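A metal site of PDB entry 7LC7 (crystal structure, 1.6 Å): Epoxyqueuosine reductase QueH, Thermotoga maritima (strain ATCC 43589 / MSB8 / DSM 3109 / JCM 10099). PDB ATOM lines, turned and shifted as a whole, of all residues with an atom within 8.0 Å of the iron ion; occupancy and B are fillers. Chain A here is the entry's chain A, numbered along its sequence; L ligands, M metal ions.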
ATOM      1  N   HIS A   7      -1.380 -25.914 -18.588  1.00  0.00           N
ATOM      2  CA  HIS A   7      -1.056 -24.915 -19.595  1.00  0.00           C
ATOM      3  C   HIS A   7      -2.278 -24.065 -19.913  1.00  0.00           C
ATOM      4  O   HIS A   7      -3.390 -24.579 -20.036  1.00  0.00           O
ATOM      5  CB  HIS A   7      -0.550 -25.608 -20.857  1.00  0.00           C
ATOM      6  CG  HIS A   7      -0.559 -24.726 -22.063  1.00  0.00           C
ATOM      7  ND1 HIS A   7      -1.557 -24.762 -23.008  1.00  0.00           N
ATOM      8  CD2 HIS A   7       0.294 -23.745 -22.439  1.00  0.00           C
ATOM      9  CE1 HIS A   7      -1.308 -23.851 -23.931  1.00  0.00           C
ATOM     10  NE2 HIS A   7      -0.184 -23.230 -23.610  1.00  0.00           N
ATOM     11  N   VAL A   8      -2.082 -22.747 -20.034  1.00  0.00           N
ATOM     12  CA  VAL A   8      -3.171 -21.832 -20.373  1.00  0.00           C
ATOM     13  C   VAL A   8      -2.880 -21.211 -21.727  1.00  0.00           C
ATOM     14  O   VAL A   8      -1.845 -20.558 -21.908  1.00  0.00           O
ATOM     15  CB  VAL A   8      -3.375 -20.732 -19.313  1.00  0.00           C
ATOM     16  CG1 VAL A   8      -4.487 -19.751 -19.762  1.00  0.00           C
ATOM     17  CG2 VAL A   8      -3.735 -21.329 -17.963  1.00  0.00           C
ATOM     18  N   CYS A   9      -3.809 -21.418 -22.678  1.00  0.00           N
ATOM     19  CA  CYS A   9      -3.729 -20.767 -23.991  1.00  0.00           C
ATOM     20  C   CYS A   9      -4.300 -19.353 -23.957  1.00  0.00           C
ATOM     21  O   CYS A   9      -3.717 -18.435 -24.557  1.00  0.00           O
ATOM     22  CB  CYS A   9      -4.481 -21.604 -25.043  1.00  0.00           C
ATOM     23  SG  CYS A   9      -6.113 -22.211 -24.556  1.00  0.00           S
ATOM     24  N   CYS A  10      -5.451 -19.142 -23.322  1.00  0.00           N
ATOM     25  CA  CYS A  10      -6.097 -17.845 -23.343  1.00  0.00           C
ATOM     26  C   CYS A  10      -7.084 -17.787 -22.184  1.00  0.00           C
ATOM     27  O   CYS A  10      -7.437 -18.807 -21.596  1.00  0.00           O
ATOM     28  CB  CYS A  10      -6.818 -17.587 -24.662  1.00  0.00           C
ATOM     29  SG  CYS A  10      -8.246 -18.652 -24.892  1.00  0.00           S
ATOM     30  N   ALA A  11      -7.482 -16.575 -21.858  1.00  0.00           N
ATOM     31  CA  ALA A  11      -8.378 -16.356 -20.732  1.00  0.00           C
ATOM     32  C   ALA A  11      -9.757 -16.957 -20.940  1.00  0.00           C
ATOM     33  O   ALA A  11     -10.335 -17.501 -19.983  1.00  0.00           O
ATOM     34  CB  ALA A  11      -8.504 -14.853 -20.436  1.00  0.00           C
ATOM     35  N   PRO A  12     -10.376 -16.834 -22.124  1.00  0.00           N
ATOM     36  CA  PRO A  12     -11.686 -17.479 -22.315  1.00  0.00           C
ATOM     37  C   PRO A  12     -11.644 -18.977 -22.041  1.00  0.00           C
ATOM     38  O   PRO A  12     -12.558 -19.497 -21.379  1.00  0.00           O
ATOM     39  CB  PRO A  12     -12.019 -17.156 -23.781  1.00  0.00           C
ATOM     40  CG  PRO A  12     -11.332 -15.848 -24.031  1.00  0.00           C
ATOM     41  CD  PRO A  12     -10.025 -15.985 -23.293  1.00  0.00           C
ATOM     42  N   ASP A  13     -10.604 -19.668 -22.501  1.00  0.00           N
ATOM     43  CA  ASP A  13     -10.540 -21.103 -22.254  1.00  0.00           C
ATOM     44  C   ASP A  13     -10.165 -21.404 -20.819  1.00  0.00           C
ATOM     45  O   ASP A  13     -10.552 -22.442 -20.274  1.00  0.00           O
ATOM     46  CB  ASP A  13      -9.566 -21.773 -23.229  1.00  0.00           C
ATOM     47  CG  ASP A  13     -10.055 -21.683 -24.674  1.00  0.00           C
ATOM     48  OD1 ASP A  13     -11.293 -21.708 -24.885  1.00  0.00           O
ATOM     49  OD2 ASP A  13      -9.207 -21.620 -25.586  1.00  0.00           O
ATOM     50  N   LEU A  14      -9.421 -20.496 -20.185  1.00  0.00           N
ATOM     51  CA  LEU A  14      -9.189 -20.645 -18.744  1.00  0.00           C
ATOM     52  C   LEU A  14     -10.490 -20.561 -17.988  1.00  0.00           C
ATOM     53  O   LEU A  14     -10.722 -21.344 -17.051  1.00  0.00           O
ATOM     54  CB  LEU A  14      -8.227 -19.555 -18.270  1.00  0.00           C
ATOM     55  CG  LEU A  14      -7.937 -19.476 -16.780  1.00  0.00           C
ATOM     56  CD1 LEU A  14      -7.320 -20.767 -16.266  1.00  0.00           C
ATOM     57  CD2 LEU A  14      -7.007 -18.269 -16.514  1.00  0.00           C
ATOM     58  N   PHE A  28       1.032 -20.053 -18.153  1.00  0.00           N
ATOM     59  CA  PHE A  28       0.784 -19.310 -19.391  1.00  0.00           C
ATOM     60  C   PHE A  28       2.085 -19.296 -20.202  1.00  0.00           C
ATOM     61  O   PHE A  28       3.008 -18.537 -19.912  1.00  0.00           O
ATOM     62  CB  PHE A  28       0.285 -17.901 -19.095  1.00  0.00           C
ATOM     63  CG  PHE A  28      -0.117 -17.145 -20.332  1.00  0.00           C
ATOM     64  CD1 PHE A  28      -1.360 -17.330 -20.912  1.00  0.00           C
ATOM     65  CD2 PHE A  28       0.780 -16.264 -20.926  1.00  0.00           C
ATOM     66  CE1 PHE A  28      -1.729 -16.630 -22.056  1.00  0.00           C
ATOM     67  CE2 PHE A  28       0.420 -15.567 -22.066  1.00  0.00           C
ATOM     68  CZ  PHE A  28      -0.817 -15.744 -22.626  1.00  0.00           C
ATOM     69  N   ASN A  30       3.074 -19.423 -24.363  1.00  0.00           N
ATOM     70  CA  ASN A  30       2.533 -19.426 -25.729  1.00  0.00           C
ATOM     71  C   ASN A  30       3.419 -18.596 -26.645  1.00  0.00           C
ATOM     72  O   ASN A  30       2.993 -17.551 -27.165  1.00  0.00           O
ATOM     73  CB  ASN A  30       1.099 -18.878 -25.754  1.00  0.00           C
ATOM     74  CG  ASN A  30       0.136 -19.672 -24.900  1.00  0.00           C
ATOM     75  OD1 ASN A  30      -0.345 -20.710 -25.314  1.00  0.00           O
ATOM     76  ND2 ASN A  30      -0.140 -19.168 -23.690  1.00  0.00           N
ATOM     77  N   ILE A  33       2.091 -17.228 -30.066  1.00  0.00           N
ATOM     78  CA  ILE A  33       1.283 -16.037 -30.251  1.00  0.00           C
ATOM     79  C   ILE A  33       2.175 -14.907 -30.734  1.00  0.00           C
ATOM     80  O   ILE A  33       3.111 -14.488 -30.038  1.00  0.00           O
ATOM     81  CB  ILE A  33       0.559 -15.635 -28.975  1.00  0.00           C
ATOM     82  CG1 ILE A  33      -0.422 -16.711 -28.531  1.00  0.00           C
ATOM     83  CG2 ILE A  33      -0.174 -14.301 -29.195  1.00  0.00           C
ATOM     84  CD1 ILE A  33      -1.002 -16.467 -27.159  1.00  0.00           C
ATOM     85  N   ARG A  42      -3.288 -10.902 -24.608  1.00  0.00           N
ATOM     86  CA  ARG A  42      -3.825 -12.158 -24.099  1.00  0.00           C
ATOM     87  C   ARG A  42      -3.354 -12.438 -22.687  1.00  0.00           C
ATOM     88  O   ARG A  42      -4.126 -12.920 -21.842  1.00  0.00           O
ATOM     89  CB  ARG A  42      -3.456 -13.298 -25.042  1.00  0.00           C
ATOM     90  CG  ARG A  42      -4.178 -13.144 -26.363  1.00  0.00           C
ATOM     91  CD  ARG A  42      -4.251 -14.409 -27.162  1.00  0.00           C
ATOM     92  NE  ARG A  42      -4.547 -14.093 -28.557  1.00  0.00           N
ATOM     93  CZ  ARG A  42      -4.615 -14.983 -29.551  1.00  0.00           C
ATOM     94  NH1 ARG A  42      -4.431 -16.290 -29.298  1.00  0.00           N
ATOM     95  NH2 ARG A  42      -4.888 -14.572 -30.786  1.00  0.00           N
ATOM     96  N   THR A 112      -4.055 -28.957 -20.142  1.00  0.00           N
ATOM     97  CA  THR A 112      -4.058 -27.707 -20.888  1.00  0.00           C
ATOM     98  C   THR A 112      -5.478 -27.208 -21.073  1.00  0.00           C
ATOM     99  O   THR A 112      -6.414 -28.002 -21.280  1.00  0.00           O
ATOM    100  CB  THR A 112      -3.389 -27.883 -22.255  1.00  0.00           C
ATOM    101  OG1 THR A 112      -3.618 -26.724 -23.052  1.00  0.00           O
ATOM    102  CG2 THR A 112      -4.028 -29.072 -23.021  1.00  0.00           C
ATOM    103  N   THR A 113      -5.643 -25.877 -21.021  1.00  0.00           N
ATOM    104  CA  THR A 113      -6.945 -25.282 -21.301  1.00  0.00           C
ATOM    105  C   THR A 113      -7.335 -25.396 -22.772  1.00  0.00           C
ATOM    106  O   THR A 113      -8.473 -25.067 -23.122  1.00  0.00           O
ATOM    107  CB  THR A 113      -6.985 -23.804 -20.850  1.00  0.00           C
ATOM    108  OG1 THR A 113      -6.026 -23.017 -21.565  1.00  0.00           O
ATOM    109  CG2 THR A 113      -6.687 -23.661 -19.353  1.00  0.00           C
ATOM    110  N   LEU A 114      -6.419 -25.835 -23.634  1.00  0.00           N
ATOM    111  CA  LEU A 114      -6.792 -26.109 -25.030  1.00  0.00           C
ATOM    112  C   LEU A 114      -7.885 -27.155 -25.092  1.00  0.00           C
ATOM    113  O   LEU A 114      -8.658 -27.191 -26.059  1.00  0.00           O
ATOM    114  CB  LEU A 114      -5.566 -26.562 -25.828  1.00  0.00           C
ATOM    115  CG  LEU A 114      -4.462 -25.530 -26.110  1.00  0.00           C
ATOM    116  CD1 LEU A 114      -3.204 -26.242 -26.567  1.00  0.00           C
ATOM    117  CD2 LEU A 114      -4.940 -24.544 -27.163  1.00  0.00           C
ATOM    118  N   LEU A 115      -7.964 -28.013 -24.065  1.00  0.00           N
ATOM    119  CA  LEU A 115      -9.060 -28.986 -24.006  1.00  0.00           C
ATOM    120  C   LEU A 115     -10.418 -28.326 -23.874  1.00  0.00           C
ATOM    121  O   LEU A 115     -11.436 -28.990 -24.074  1.00  0.00           O
ATOM    122  CB  LEU A 115      -8.839 -29.922 -22.836  1.00  0.00           C
ATOM    123  CG  LEU A 115      -7.686 -30.899 -22.983  1.00  0.00           C
ATOM    124  CD1 LEU A 115      -7.466 -31.616 -21.683  1.00  0.00           C
ATOM    125  CD2 LEU A 115      -7.971 -31.908 -24.130  1.00  0.00           C
ATOM    126  N   ALA A 116     -10.475 -27.032 -23.534  1.00  0.00           N
ATOM    127  CA  ALA A 116     -11.737 -26.313 -23.449  1.00  0.00           C
ATOM    128  C   ALA A 116     -12.053 -25.551 -24.724  1.00  0.00           C
ATOM    129  O   ALA A 116     -13.135 -24.952 -24.821  1.00  0.00           O
ATOM    130  CB  ALA A 116     -11.694 -25.317 -22.275  1.00  0.00           C
ATOM    131  N   SER A 117     -11.168 -25.542 -25.690  1.00  0.00           N
ATOM    132  CA  SER A 117     -11.390 -24.705 -26.854  1.00  0.00           C
ATOM    133  C   SER A 117     -12.325 -25.416 -27.827  1.00  0.00           C
ATOM    134  O   SER A 117     -12.102 -26.579 -28.155  1.00  0.00           O
ATOM    135  CB  SER A 117     -10.071 -24.378 -27.533  1.00  0.00           C
ATOM    136  OG  SER A 117     -10.295 -23.957 -28.877  1.00  0.00           O
ATOM    137  N   PRO A 118     -13.386 -24.754 -28.306  1.00  0.00           N
ATOM    138  CA  PRO A 118     -14.316 -25.445 -29.219  1.00  0.00           C
ATOM    139  C   PRO A 118     -13.719 -25.738 -30.592  1.00  0.00           C
ATOM    140  O   PRO A 118     -14.249 -26.608 -31.301  1.00  0.00           O
ATOM    141  CB  PRO A 118     -15.500 -24.472 -29.333  1.00  0.00           C
ATOM    142  CG  PRO A 118     -15.268 -23.421 -28.298  1.00  0.00           C
ATOM    143  CD  PRO A 118     -13.806 -23.378 -28.011  1.00  0.00           C
ATOM    144  N   LYS A 120     -10.492 -26.828 -31.218  1.00  0.00           N
ATOM    145  CA  LYS A 120      -9.395 -27.776 -31.260  1.00  0.00           C
ATOM    146  C   LYS A 120      -9.895 -29.213 -31.380  1.00  0.00           C
ATOM    147  O   LYS A 120     -11.056 -29.542 -31.148  1.00  0.00           O
ATOM    148  CB  LYS A 120      -8.507 -27.608 -30.020  1.00  0.00           C
ATOM    149  CG  LYS A 120      -7.915 -26.206 -29.848  1.00  0.00           C
ATOM    150  CD  LYS A 120      -6.739 -25.967 -30.775  1.00  0.00           C
ATOM    151  CE  LYS A 120      -6.804 -24.586 -31.426  1.00  0.00           C
ATOM    152  NZ  LYS A 120      -7.360 -23.536 -30.515  1.00  0.00           N
ATOM    153  N   GLN A 166     -10.254 -13.367 -28.407  1.00  0.00           N
ATOM    154  CA  GLN A 166      -9.552 -13.256 -29.671  1.00  0.00           C
ATOM    155  C   GLN A 166     -10.319 -13.938 -30.807  1.00  0.00           C
ATOM    156  O   GLN A 166     -11.216 -14.757 -30.574  1.00  0.00           O
ATOM    157  CB  GLN A 166      -8.151 -13.841 -29.566  1.00  0.00           C
ATOM    158  CG  GLN A 166      -8.121 -15.360 -29.475  1.00  0.00           C
ATOM    159  CD  GLN A 166      -8.176 -15.868 -28.047  1.00  0.00           C
ATOM    160  OE1 GLN A 166      -8.535 -15.141 -27.114  1.00  0.00           O
ATOM    161  NE2 GLN A 166      -7.823 -17.134 -27.865  1.00  0.00           N
ATOM    162  N   TYR A 168      -8.430 -15.198 -33.680  1.00  0.00           N
ATOM    163  CA  TYR A 168      -7.540 -16.076 -34.430  1.00  0.00           C
ATOM    164  C   TYR A 168      -6.711 -16.876 -33.444  1.00  0.00           C
ATOM    165  O   TYR A 168      -6.477 -16.430 -32.312  1.00  0.00           O
ATOM    166  CB  TYR A 168      -6.653 -15.307 -35.427  1.00  0.00           C
ATOM    167  CG  TYR A 168      -5.546 -14.441 -34.859  1.00  0.00           C
ATOM    168  CD1 TYR A 168      -5.830 -13.252 -34.192  1.00  0.00           C
ATOM    169  CD2 TYR A 168      -4.214 -14.780 -35.044  1.00  0.00           C
ATOM    170  CE1 TYR A 168      -4.808 -12.453 -33.692  1.00  0.00           C
ATOM    171  CE2 TYR A 168      -3.191 -13.987 -34.552  1.00  0.00           C
ATOM    172  CZ  TYR A 168      -3.492 -12.815 -33.888  1.00  0.00           C
ATOM    173  OH  TYR A 168      -2.457 -12.036 -33.409  1.00  0.00           O
ATOM    174  N   CYS A 169      -6.279 -18.057 -33.882  1.00  0.00           N
ATOM    175  CA  CYS A 169      -5.717 -19.025 -32.938  1.00  0.00           C
ATOM    176  C   CYS A 169      -4.517 -18.452 -32.203  1.00  0.00           C
ATOM    177  O   CYS A 169      -4.417 -18.544 -30.972  1.00  0.00           O
ATOM    178  CB  CYS A 169      -5.351 -20.308 -33.661  1.00  0.00           C
ATOM    179  SG  CYS A 169      -5.089 -21.616 -32.487  1.00  0.00           S
HETATM  180 CL1  LIG L   1      -6.888 -20.606 -27.798  1.00  0.00          CL
HETATM  181 FE    FE M   1      -7.502 -20.719 -25.673  1.00  0.00          FE
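The iron ion is bound by OD2 of Asp 13 (1.9 Å), CL1 of the ligand (2.2 Å), SG of Cys 9 (2.3 Å) and SG of Cys 10 (2.3 Å). The iron ion has four donor atoms within binding distance.
The side-chain sulfur of Cys 10 lies close to the side-chain amide nitrogen of Gln 166 (3.4 Å). N of Cys 9 is in hydrogen-bond range of OG1 of Thr 113 (3.0 Å). The side-chain sulfur of Cys 9 lies close to the backbone NH of Leu 114, at 3.8 Å.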
